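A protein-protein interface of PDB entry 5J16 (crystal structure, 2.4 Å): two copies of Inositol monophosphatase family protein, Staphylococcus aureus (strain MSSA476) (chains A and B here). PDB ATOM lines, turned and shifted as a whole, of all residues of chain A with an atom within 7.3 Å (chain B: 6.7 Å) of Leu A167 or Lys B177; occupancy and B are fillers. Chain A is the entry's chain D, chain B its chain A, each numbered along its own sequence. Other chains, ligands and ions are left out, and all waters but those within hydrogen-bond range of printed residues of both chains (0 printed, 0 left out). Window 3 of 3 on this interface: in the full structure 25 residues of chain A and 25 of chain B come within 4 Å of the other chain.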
ATOM      1  N   ILE A 162      28.953  11.591  -5.714  1.00  0.00           N
ATOM      2  CA  ILE A 162      27.739  12.341  -5.419  1.00  0.00           C
ATOM      3  C   ILE A 162      26.655  12.139  -6.492  1.00  0.00           C
ATOM      4  O   ILE A 162      26.913  12.241  -7.690  1.00  0.00           O
ATOM      5  CB  ILE A 162      28.038  13.821  -5.139  1.00  0.00           C
ATOM      6  CG1 ILE A 162      26.730  14.599  -4.985  1.00  0.00           C
ATOM      7  CG2 ILE A 162      28.927  14.444  -6.205  1.00  0.00           C
ATOM      8  CD1 ILE A 162      26.920  15.946  -4.319  1.00  0.00           C
ATOM      9  N   ASN A 163      25.438  11.825  -6.055  1.00  0.00           N
ATOM     10  CA  ASN A 163      24.388  11.572  -6.995  1.00  0.00           C
ATOM     11  C   ASN A 163      23.869  12.875  -7.631  1.00  0.00           C
ATOM     12  O   ASN A 163      23.681  13.889  -6.928  1.00  0.00           O
ATOM     13  CB  ASN A 163      23.232  10.828  -6.366  1.00  0.00           C
ATOM     14  CG  ASN A 163      22.345  10.170  -7.417  1.00  0.00           C
ATOM     15  OD1 ASN A 163      21.530  10.838  -8.050  1.00  0.00           O
ATOM     16  ND2 ASN A 163      22.541   8.873  -7.643  1.00  0.00           N
ATOM     17  N   PRO A 164      23.621  12.848  -8.954  1.00  0.00           N
ATOM     18  CA  PRO A 164      23.044  13.990  -9.613  1.00  0.00           C
ATOM     19  C   PRO A 164      21.752  14.483  -8.985  1.00  0.00           C
ATOM     20  O   PRO A 164      21.496  15.674  -9.031  1.00  0.00           O
ATOM     21  CB  PRO A 164      22.763  13.473 -11.026  1.00  0.00           C
ATOM     22  CG  PRO A 164      23.808  12.462 -11.247  1.00  0.00           C
ATOM     23  CD  PRO A 164      23.945  11.780  -9.921  1.00  0.00           C
ATOM     24  N   ASN A 165      20.947  13.605  -8.388  1.00  0.00           N
ATOM     25  CA  ASN A 165      19.709  14.044  -7.738  1.00  0.00           C
ATOM     26  C   ASN A 165      19.910  15.135  -6.700  1.00  0.00           C
ATOM     27  O   ASN A 165      19.064  15.992  -6.546  1.00  0.00           O
ATOM     28  CB  ASN A 165      18.959  12.852  -7.149  1.00  0.00           C
ATOM     29  CG  ASN A 165      18.271  12.023  -8.239  1.00  0.00           C
ATOM     30  OD1 ASN A 165      17.338  12.522  -8.886  1.00  0.00           O
ATOM     31  ND2 ASN A 165      18.747  10.765  -8.479  1.00  0.00           N
ATOM     32  N   TRP A 166      21.035  15.127  -6.013  1.00  0.00           N
ATOM     33  CA  TRP A 166      21.277  16.139  -4.992  1.00  0.00           C
ATOM     34  C   TRP A 166      21.643  17.477  -5.581  1.00  0.00           C
ATOM     35  O   TRP A 166      21.483  18.484  -4.920  1.00  0.00           O
ATOM     36  CB  TRP A 166      22.340  15.690  -3.976  1.00  0.00           C
ATOM     37  CG  TRP A 166      22.057  14.358  -3.492  1.00  0.00           C
ATOM     38  CD1 TRP A 166      22.855  13.272  -3.601  1.00  0.00           C
ATOM     39  CD2 TRP A 166      20.839  13.919  -2.896  1.00  0.00           C
ATOM     40  NE1 TRP A 166      22.230  12.161  -3.078  1.00  0.00           N
ATOM     41  CE2 TRP A 166      20.990  12.531  -2.618  1.00  0.00           C
ATOM     42  CE3 TRP A 166      19.652  14.568  -2.505  1.00  0.00           C
ATOM     43  CZ2 TRP A 166      19.994  11.769  -1.971  1.00  0.00           C
ATOM     44  CZ3 TRP A 166      18.636  13.792  -1.859  1.00  0.00           C
ATOM     45  CH2 TRP A 166      18.828  12.408  -1.606  1.00  0.00           C
ATOM     46  N   LEU A 167      22.119  17.499  -6.814  1.00  0.00           N
ATOM     47  CA  LEU A 167      22.422  18.776  -7.471  1.00  0.00           C
ATOM     48  C   LEU A 167      21.188  19.642  -7.839  1.00  0.00           C
ATOM     49  O   LEU A 167      21.332  20.839  -8.093  1.00  0.00           O
ATOM     50  CB  LEU A 167      23.271  18.529  -8.711  1.00  0.00           C
ATOM     51  CG  LEU A 167      24.760  18.353  -8.480  1.00  0.00           C
ATOM     52  CD1 LEU A 167      25.368  19.715  -8.274  1.00  0.00           C
ATOM     53  CD2 LEU A 167      25.104  17.436  -7.320  1.00  0.00           C
ATOM     54  N   THR A 168      20.012  19.014  -7.899  1.00  0.00           N
ATOM     55  CA  THR A 168      18.793  19.632  -8.415  1.00  0.00           C
ATOM     56  C   THR A 168      17.920  20.228  -7.317  1.00  0.00           C
ATOM     57  O   THR A 168      16.974  20.961  -7.601  1.00  0.00           O
ATOM     58  CB  THR A 168      17.889  18.572  -9.064  1.00  0.00           C
ATOM     59  OG1 THR A 168      17.333  17.767  -8.016  1.00  0.00           O
ATOM     60  CG2 THR A 168      18.673  17.719 -10.088  1.00  0.00           C
ATOM     61  N   LYS A 169      18.192  19.835  -6.080  1.00  0.00           N
ATOM     62  CA  LYS A 169      17.416  20.252  -4.911  1.00  0.00           C
ATOM     63  C   LYS A 169      17.725  21.702  -4.586  1.00  0.00           C
ATOM     64  O   LYS A 169      18.898  22.070  -4.655  1.00  0.00           O
ATOM     65  CB  LYS A 169      17.731  19.355  -3.676  1.00  0.00           C
ATOM     66  CG  LYS A 169      16.710  18.255  -3.428  1.00  0.00           C
ATOM     67  CD  LYS A 169      16.718  17.153  -4.477  1.00  0.00           C
ATOM     68  CE  LYS A 169      15.346  16.476  -4.589  1.00  0.00           C
ATOM     69  NZ  LYS A 169      15.415  15.000  -4.838  1.00  0.00           N
ATOM     70  N   PRO A 170      16.691  22.500  -4.204  1.00  0.00           N
ATOM     71  CA  PRO A 170      16.761  23.954  -3.929  1.00  0.00           C
ATOM     72  C   PRO A 170      18.053  24.497  -3.255  1.00  0.00           C
ATOM     73  O   PRO A 170      18.852  25.145  -3.941  1.00  0.00           O
ATOM     74  CB  PRO A 170      15.525  24.212  -3.031  1.00  0.00           C
ATOM     75  CG  PRO A 170      14.942  22.868  -2.719  1.00  0.00           C
ATOM     76  CD  PRO A 170      15.355  21.985  -3.850  1.00  0.00           C
ATOM     77  N   LEU A 172      20.460  22.625  -1.208  1.00  0.00           N
ATOM     78  CA  LEU A 172      21.469  21.588  -1.458  1.00  0.00           C
ATOM     79  C   LEU A 172      22.312  21.795  -2.735  1.00  0.00           C
ATOM     80  O   LEU A 172      23.552  21.742  -2.696  1.00  0.00           O
ATOM     81  CB  LEU A 172      20.770  20.231  -1.610  1.00  0.00           C
ATOM     82  CG  LEU A 172      20.620  19.374  -0.367  1.00  0.00           C
ATOM     83  CD1 LEU A 172      19.893  18.082  -0.747  1.00  0.00           C
ATOM     84  CD2 LEU A 172      21.992  19.128   0.258  1.00  0.00           C
ATOM     85  N   GLY A 173      21.605  21.999  -3.856  1.00  0.00           N
ATOM     86  CA  GLY A 173      22.224  22.194  -5.156  1.00  0.00           C
ATOM     87  C   GLY A 173      23.355  23.188  -5.118  1.00  0.00           C
ATOM     88  O   GLY A 173      24.480  22.862  -5.507  1.00  0.00           O
ATOM     89  N   GLU A 174      23.065  24.385  -4.603  1.00  0.00           N
ATOM     90  CA  GLU A 174      24.039  25.463  -4.593  1.00  0.00           C
ATOM     91  C   GLU A 174      25.204  25.169  -3.620  1.00  0.00           C
ATOM     92  O   GLU A 174      26.355  25.495  -3.938  1.00  0.00           O
ATOM     93  CB  GLU A 174      23.359  26.821  -4.337  1.00  0.00           C
ATOM     94  N   ILE A 175      24.932  24.520  -2.478  1.00  0.00           N
ATOM     95  CA  ILE A 175      26.009  24.090  -1.583  1.00  0.00           C
ATOM     96  C   ILE A 175      26.862  23.053  -2.313  1.00  0.00           C
ATOM     97  O   ILE A 175      28.093  23.141  -2.297  1.00  0.00           O
ATOM     98  CB  ILE A 175      25.510  23.517  -0.236  1.00  0.00           C
ATOM     99  N   PHE A 176      26.236  22.102  -3.002  1.00  0.00           N
ATOM    100  CA  PHE A 176      27.031  21.042  -3.630  1.00  0.00           C
ATOM    101  C   PHE A 176      27.690  21.443  -4.940  1.00  0.00           C
ATOM    102  O   PHE A 176      28.703  20.871  -5.274  1.00  0.00           O
ATOM    103  CB  PHE A 176      26.242  19.736  -3.811  1.00  0.00           C
ATOM    104  CG  PHE A 176      26.095  18.919  -2.558  1.00  0.00           C
ATOM    105  CD1 PHE A 176      27.167  18.684  -1.719  1.00  0.00           C
ATOM    106  CD2 PHE A 176      24.886  18.333  -2.254  1.00  0.00           C
ATOM    107  CE1 PHE A 176      27.032  17.901  -0.578  1.00  0.00           C
ATOM    108  CE2 PHE A 176      24.737  17.562  -1.117  1.00  0.00           C
ATOM    109  CZ  PHE A 176      25.813  17.343  -0.279  1.00  0.00           C
ATOM    110  N   LYS A 177      27.122  22.410  -5.676  1.00  0.00           N
ATOM    111  CA  LYS A 177      27.708  22.893  -6.941  1.00  0.00           C
ATOM    112  C   LYS A 177      29.193  23.197  -6.841  1.00  0.00           C
ATOM    113  O   LYS A 177      29.967  22.804  -7.727  1.00  0.00           O
ATOM    114  CB  LYS A 177      26.984  24.150  -7.451  1.00  0.00           C
ATOM    115  N   GLU A 178      29.601  23.879  -5.769  1.00  0.00           N
ATOM    116  CA  GLU A 178      30.980  24.423  -5.704  1.00  0.00           C
ATOM    117  C   GLU A 178      31.970  23.246  -5.547  1.00  0.00           C
ATOM    118  O   GLU A 178      32.999  23.174  -6.224  1.00  0.00           O
ATOM    119  CB  GLU A 178      31.122  25.591  -4.674  1.00  0.00           C
ATOM    120  N   ILE A 179      31.587  22.285  -4.718  1.00  0.00           N
ATOM    121  CA  ILE A 179      32.380  21.074  -4.474  1.00  0.00           C
ATOM    122  C   ILE A 179      32.552  20.185  -5.725  1.00  0.00           C
ATOM    123  O   ILE A 179      33.657  19.684  -5.997  1.00  0.00           O
ATOM    124  CB  ILE A 179      31.865  20.300  -3.200  1.00  0.00           C
ATOM    125  CG1 ILE A 179      32.680  19.044  -2.932  1.00  0.00           C
ATOM    126  CG2 ILE A 179      30.442  19.851  -3.299  1.00  0.00           C
ATOM    127  CD1 ILE A 179      33.992  19.397  -2.305  1.00  0.00           C
ATOM    128  N   VAL A 180      31.471  20.045  -6.489  1.00  0.00           N
ATOM    129  CA  VAL A 180      31.486  19.337  -7.775  1.00  0.00           C
ATOM    130  C   VAL A 180      32.375  20.052  -8.786  1.00  0.00           C
ATOM    131  O   VAL A 180      33.109  19.411  -9.523  1.00  0.00           O
ATOM    132  CB  VAL A 180      30.059  19.205  -8.379  1.00  0.00           C
ATOM    133  CG1 VAL A 180      30.087  18.687  -9.828  1.00  0.00           C
ATOM    134  CG2 VAL A 180      29.182  18.303  -7.512  1.00  0.00           C
ATOM    135  N   ASN A 181      32.290  21.382  -8.824  1.00  0.00           N
ATOM    136  CA  ASN A 181      33.106  22.177  -9.747  1.00  0.00           C
ATOM    137  C   ASN A 181      34.587  22.074  -9.430  1.00  0.00           C
ATOM    138  O   ASN A 181      35.380  21.913 -10.348  1.00  0.00           O
ATOM    139  CB  ASN A 181      32.637  23.635  -9.783  1.00  0.00           C
ATOM    140  CG  ASN A 181      31.314  23.822 -10.571  1.00  0.00           C
ATOM    141  OD1 ASN A 181      31.007  23.081 -11.511  1.00  0.00           O
ATOM    142  ND2 ASN A 181      30.530  24.817 -10.178  1.00  0.00           N
ATOM    143  N   ILE B 162      24.228  10.278 -16.416  1.00  0.00           N
ATOM    144  CA  ILE B 162      24.623  11.663 -16.548  1.00  0.00           C
ATOM    145  C   ILE B 162      25.502  12.162 -15.431  1.00  0.00           C
ATOM    146  O   ILE B 162      25.190  12.033 -14.262  1.00  0.00           O
ATOM    147  CB  ILE B 162      23.380  12.563 -16.621  1.00  0.00           C
ATOM    148  CG1 ILE B 162      23.764  13.983 -17.011  1.00  0.00           C
ATOM    149  CG2 ILE B 162      22.568  12.512 -15.337  1.00  0.00           C
ATOM    150  CD1 ILE B 162      22.536  14.861 -17.181  1.00  0.00           C
ATOM    151  N   PRO B 164      27.209  14.568 -12.662  1.00  0.00           N
ATOM    152  CA  PRO B 164      26.925  15.765 -11.886  1.00  0.00           C
ATOM    153  C   PRO B 164      27.494  17.059 -12.470  1.00  0.00           C
ATOM    154  O   PRO B 164      26.907  18.113 -12.286  1.00  0.00           O
ATOM    155  CB  PRO B 164      27.623  15.476 -10.547  1.00  0.00           C
ATOM    156  CG  PRO B 164      27.544  14.023 -10.421  1.00  0.00           C
ATOM    157  CD  PRO B 164      27.719  13.490 -11.790  1.00  0.00           C
ATOM    158  N   ASN B 165      28.648  16.995 -13.127  1.00  0.00           N
ATOM    159  CA  ASN B 165      29.265  18.213 -13.638  1.00  0.00           C
ATOM    160  C   ASN B 165      28.367  19.009 -14.614  1.00  0.00           C
ATOM    161  O   ASN B 165      28.364  20.228 -14.585  1.00  0.00           O
ATOM    162  CB  ASN B 165      30.669  17.918 -14.186  1.00  0.00           C
ATOM    163  CG  ASN B 165      31.669  17.566 -13.060  1.00  0.00           C
ATOM    164  OD1 ASN B 165      32.107  18.455 -12.319  1.00  0.00           O
ATOM    165  ND2 ASN B 165      32.004  16.260 -12.905  1.00  0.00           N
ATOM    166  N   TRP B 166      27.549  18.320 -15.398  1.00  0.00           N
ATOM    167  CA  TRP B 166      26.641  18.982 -16.349  1.00  0.00           C
ATOM    168  C   TRP B 166      25.528  19.760 -15.679  1.00  0.00           C
ATOM    169  O   TRP B 166      25.012  20.687 -16.280  1.00  0.00           O
ATOM    170  CB  TRP B 166      26.048  17.984 -17.404  1.00  0.00           C
ATOM    171  CG  TRP B 166      27.100  17.194 -18.022  1.00  0.00           C
ATOM    172  CD1 TRP B 166      27.164  15.831 -18.108  1.00  0.00           C
ATOM    173  CD2 TRP B 166      28.336  17.694 -18.537  1.00  0.00           C
ATOM    174  NE1 TRP B 166      28.348  15.450 -18.694  1.00  0.00           N
ATOM    175  CE2 TRP B 166      29.093  16.572 -18.959  1.00  0.00           C
ATOM    176  CE3 TRP B 166      28.866  18.981 -18.716  1.00  0.00           C
ATOM    177  CZ2 TRP B 166      30.356  16.697 -19.566  1.00  0.00           C
ATOM    178  CZ3 TRP B 166      30.121  19.106 -19.310  1.00  0.00           C
ATOM    179  CH2 TRP B 166      30.853  17.966 -19.735  1.00  0.00           C
ATOM    180  N   LEU B 167      25.168  19.390 -14.456  1.00  0.00           N
ATOM    181  CA  LEU B 167      24.045  19.991 -13.771  1.00  0.00           C
ATOM    182  C   LEU B 167      24.385  21.349 -13.167  1.00  0.00           C
ATOM    183  O   LEU B 167      23.481  22.086 -12.791  1.00  0.00           O
ATOM    184  CB  LEU B 167      23.486  19.042 -12.702  1.00  0.00           C
ATOM    185  CG  LEU B 167      22.501  18.017 -13.249  1.00  0.00           C
ATOM    186  CD1 LEU B 167      23.192  17.086 -14.247  1.00  0.00           C
ATOM    187  CD2 LEU B 167      21.823  17.242 -12.125  1.00  0.00           C
ATOM    188  N   THR B 168      25.674  21.662 -13.073  1.00  0.00           N
ATOM    189  CA  THR B 168      26.163  22.936 -12.532  1.00  0.00           C
ATOM    190  C   THR B 168      26.382  23.978 -13.629  1.00  0.00           C
ATOM    191  O   THR B 168      26.937  25.015 -13.352  1.00  0.00           O
ATOM    192  CB  THR B 168      27.556  22.759 -11.900  1.00  0.00           C
ATOM    193  OG1 THR B 168      28.518  22.466 -12.933  1.00  0.00           O
ATOM    194  CG2 THR B 168      27.557  21.658 -10.833  1.00  0.00           C
ATOM    195  N   LYS B 169      26.025  23.685 -14.876  1.00  0.00           N
ATOM    196  CA  LYS B 169      26.374  24.554 -15.981  1.00  0.00           C
ATOM    197  C   LYS B 169      25.275  25.550 -16.167  1.00  0.00           C
ATOM    198  O   LYS B 169      24.123  25.173 -16.016  1.00  0.00           O
ATOM    199  CB  LYS B 169      26.559  23.760 -17.266  1.00  0.00           C
ATOM    200  CG  LYS B 169      27.846  22.965 -17.258  1.00  0.00           C
ATOM    201  CD  LYS B 169      29.063  23.863 -17.463  1.00  0.00           C
ATOM    202  CE  LYS B 169      30.254  23.346 -16.689  1.00  0.00           C
ATOM    203  NZ  LYS B 169      30.588  21.961 -17.111  1.00  0.00           N
ATOM    204  N   LEU B 172      22.293  24.809 -19.502  1.00  0.00           N
ATOM    205  CA  LEU B 172      22.235  23.365 -19.673  1.00  0.00           C
ATOM    206  C   LEU B 172      21.894  22.626 -18.350  1.00  0.00           C
ATOM    207  O   LEU B 172      21.174  21.653 -18.340  1.00  0.00           O
ATOM    208  CB  LEU B 172      23.586  22.883 -20.188  1.00  0.00           C
ATOM    209  CG  LEU B 172      23.692  21.383 -20.400  1.00  0.00           C
ATOM    210  CD1 LEU B 172      22.760  20.888 -21.521  1.00  0.00           C
ATOM    211  CD2 LEU B 172      25.152  21.066 -20.656  1.00  0.00           C
ATOM    212  N   GLY B 173      22.432  23.094 -17.232  1.00  0.00           N
ATOM    213  CA  GLY B 173      22.125  22.494 -15.954  1.00  0.00           C
ATOM    214  C   GLY B 173      20.640  22.484 -15.689  1.00  0.00           C
ATOM    215  O   GLY B 173      20.074  21.454 -15.317  1.00  0.00           O
ATOM    216  N   GLU B 174      20.011  23.626 -15.926  1.00  0.00           N
ATOM    217  CA  GLU B 174      18.617  23.795 -15.600  1.00  0.00           C
ATOM    218  C   GLU B 174      17.733  22.905 -16.463  1.00  0.00           C
ATOM    219  O   GLU B 174      16.835  22.277 -15.940  1.00  0.00           O
ATOM    220  CB  GLU B 174      18.216  25.279 -15.689  1.00  0.00           C
ATOM    221  CG  GLU B 174      17.112  25.694 -14.738  1.00  0.00           C
ATOM    222  CD  GLU B 174      17.261  25.096 -13.341  1.00  0.00           C
ATOM    223  OE1 GLU B 174      18.344  25.246 -12.715  1.00  0.00           O
ATOM    224  OE2 GLU B 174      16.292  24.442 -12.889  1.00  0.00           O
ATOM    225  N   ILE B 175      18.022  22.827 -17.761  1.00  0.00           N
ATOM    226  CA  ILE B 175      17.369  21.868 -18.691  1.00  0.00           C
ATOM    227  C   ILE B 175      17.538  20.393 -18.262  1.00  0.00           C
ATOM    228  O   ILE B 175      16.568  19.621 -18.292  1.00  0.00           O
ATOM    229  CB  ILE B 175      17.884  22.039 -20.137  1.00  0.00           C
ATOM    230  CG1 ILE B 175      17.398  23.356 -20.738  1.00  0.00           C
ATOM    231  CG2 ILE B 175      17.429  20.914 -21.041  1.00  0.00           C
ATOM    232  CD1 ILE B 175      18.315  23.920 -21.816  1.00  0.00           C
ATOM    233  N   PHE B 176      18.739  19.997 -17.855  1.00  0.00           N
ATOM    234  CA  PHE B 176      18.942  18.621 -17.353  1.00  0.00           C
ATOM    235  C   PHE B 176      18.284  18.301 -15.987  1.00  0.00           C
ATOM    236  O   PHE B 176      17.974  17.145 -15.729  1.00  0.00           O
ATOM    237  CB  PHE B 176      20.435  18.254 -17.291  1.00  0.00           C
ATOM    238  CG  PHE B 176      21.065  17.880 -18.617  1.00  0.00           C
ATOM    239  CD1 PHE B 176      20.359  17.188 -19.619  1.00  0.00           C
ATOM    240  CD2 PHE B 176      22.413  18.145 -18.825  1.00  0.00           C
ATOM    241  CE1 PHE B 176      20.986  16.828 -20.812  1.00  0.00           C
ATOM    242  CE2 PHE B 176      23.053  17.768 -20.002  1.00  0.00           C
ATOM    243  CZ  PHE B 176      22.345  17.123 -21.005  1.00  0.00           C
ATOM    244  N   LYS B 177      18.064  19.292 -15.116  1.00  0.00           N
ATOM    245  CA  LYS B 177      17.440  19.014 -13.814  1.00  0.00           C
ATOM    246  C   LYS B 177      16.027  18.420 -13.915  1.00  0.00           C
ATOM    247  O   LYS B 177      15.693  17.510 -13.134  1.00  0.00           O
ATOM    248  CB  LYS B 177      17.433  20.256 -12.928  1.00  0.00           C
ATOM    249  CG  LYS B 177      18.815  20.631 -12.409  1.00  0.00           C
ATOM    250  CD  LYS B 177      18.790  21.912 -11.588  1.00  0.00           C
ATOM    251  CE  LYS B 177      20.153  22.234 -10.988  1.00  0.00           C
ATOM    252  NZ  LYS B 177      21.271  22.189 -11.979  1.00  0.00           N
ATOM    253  N   GLU B 178      15.200  18.861 -14.868  1.00  0.00           N
ATOM    254  CA  GLU B 178      13.874  18.229 -14.992  1.00  0.00           C
ATOM    255  C   GLU B 178      14.033  16.734 -15.336  1.00  0.00           C
ATOM    256  O   GLU B 178      13.348  15.888 -14.785  1.00  0.00           O
ATOM    257  CB  GLU B 178      12.985  18.880 -16.047  1.00  0.00           C
ATOM    258  CG  GLU B 178      12.620  20.336 -15.827  1.00  0.00           C
ATOM    259  CD  GLU B 178      13.273  21.238 -16.860  1.00  0.00           C
ATOM    260  OE1 GLU B 178      14.475  21.525 -16.681  1.00  0.00           O
ATOM    261  OE2 GLU B 178      12.602  21.633 -17.852  1.00  0.00           O
ATOM    262  N   ILE B 179      14.965  16.413 -16.234  1.00  0.00           N
ATOM    263  CA  ILE B 179      15.196  15.022 -16.657  1.00  0.00           C
ATOM    264  C   ILE B 179      15.694  14.181 -15.537  1.00  0.00           C
ATOM    265  O   ILE B 179      15.249  13.035 -15.369  1.00  0.00           O
ATOM    266  CB  ILE B 179      16.179  14.938 -17.840  1.00  0.00           C
ATOM    267  CG1 ILE B 179      15.500  15.514 -19.086  1.00  0.00           C
ATOM    268  CG2 ILE B 179      16.669  13.516 -18.088  1.00  0.00           C
ATOM    269  CD1 ILE B 179      16.070  16.830 -19.533  1.00  0.00           C
ATOM    270  N   VAL B 180      16.618  14.738 -14.768  1.00  0.00           N
ATOM    271  CA  VAL B 180      17.124  14.031 -13.589  1.00  0.00           C
ATOM    272  C   VAL B 180      15.978  13.735 -12.620  1.00  0.00           C
ATOM    273  O   VAL B 180      15.851  12.614 -12.187  1.00  0.00           O
ATOM    274  CB  VAL B 180      18.293  14.777 -12.913  1.00  0.00           C
ATOM    275  CG1 VAL B 180      18.744  14.027 -11.663  1.00  0.00           C
ATOM    276  CG2 VAL B 180      19.452  14.951 -13.896  1.00  0.00           C
ATOM    277  N   ASN B 181      15.109  14.715 -12.382  1.00  0.00           N
ATOM    278  CA  ASN B 181      14.009  14.592 -11.405  1.00  0.00           C
ATOM    279  C   ASN B 181      12.858  13.705 -11.826  1.00  0.00           C
ATOM    280  O   ASN B 181      12.216  13.132 -10.942  1.00  0.00           O
ATOM    281  CB  ASN B 181      13.418  15.970 -11.072  1.00  0.00           C
ATOM    282  CG  ASN B 181      14.382  16.854 -10.311  1.00  0.00           C
ATOM    283  OD1 ASN B 181      15.286  16.367  -9.658  1.00  0.00           O
ATOM    284  ND2 ASN B 181      14.175  18.158 -10.375  1.00  0.00           N
ATOM    285  N   ASP B 182      12.545  13.617 -13.128  1.00  0.00           N
ATOM    286  CA  ASP B 182      11.523  12.653 -13.603  1.00  0.00           C
ATOM    287  C   ASP B 182      12.152  11.268 -13.592  1.00  0.00           C
ATOM    288  O   ASP B 182      11.460  10.295 -13.277  1.00  0.00           O
ATOM    289  CB  ASP B 182      10.895  13.014 -14.979  1.00  0.00           C
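The side-chain amide oxygen (OD1) of Asn B165 lies close to the backbone carbonyl oxygen (O) of Val A180 (3.1 Å). OG1 of Thr B168 lies within hydrogen-bond range of OD1 of Asn A181 (2.9 Å). The side-chain hydroxyl (OG1) of Thr A168 is in hydrogen-bond range of the side-chain amide oxygen (OD1) of Asn B181.
O of Asn B165 lies within hydrogen-bond range of OG1 of Thr B168 (2.8 Å). The side-chain amide nitrogen (ND2) of Asn B181 sits close to the backbone carbonyl oxygen (O) of Lys B177. The side-chain amide oxygen (OD1) of Asn A163 is in hydrogen-bond range of the side-chain amide nitrogen (ND2) of Asn A165, at 2.8 Å. O of Asn A165 sits at hydrogen-bond distance from OG1 of Thr A168. O of Lys A177 sits at hydrogen-bond distance from ND2 of Asn A181, at 3.2 Å.
Among the printed residues, pairs that only touch across the chains: Ile A162 with Pro B164, Pro A164 with Ile B162, Pro A164 with Leu B167, Asn A165 with Val B180, Leu A167 with Leu B167, Leu A167 with Thr B168, Leu A167 with Lys B177, Thr A168 with Leu B167 and Thr A168 with Lys B177.
Leu A167 touches just these residues of chain B: Leu B167, Thr B168 and Lys B177. Of the printed residues of chain B, Thr A168 touches Leu B167, Lys B177 and Asn B181. Of the printed residues of chain A, Ile B162 touches Pro A164 (3.3 Å). Lys B177 touches just these residues of chain A: Leu A167 and Thr A168. The nearest residue of chain B that does not touch Leu A167 is Pro B164 (4.4 Å). The nearest residue of chain A that does not touch Lys B177 is Lys A169 (5.8 Å). The nearest printed residue of chain B that does not touch Asn A181 is Asn B165 (4.6 Å).
Of the 18 printed residues of chain B, 8 touch a printed residue of chain A. Printed residues of chain A that touch a printed residue of chain B: Ile A162, Pro A164, Asn A165, Leu A167, Thr A168, Val A180 and Asn A181. Among the printed residues, 12 pairs touch across the chains. Among the printed residues, no Asp or Glu carboxylate lies within 4 Å of a Lys or Arg side-chain nitrogen of the other chain.
Asn A165 touches Val B180, and with the chains exchanged Val A180 touches Asn B165. Leu B167 touches its own counterpart, Leu A167. Leu A167 touches Lys B177, but with the chains exchanged Lys A177 does not touch Leu B167 (6.7 Å). Thr A168 touches Asn B181, and with the chains exchanged Asn A181 touches Thr B168. Of the 12 pairs that touch across the chains among the printed residues, 9 have their exchanged pair printed and touching as well.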
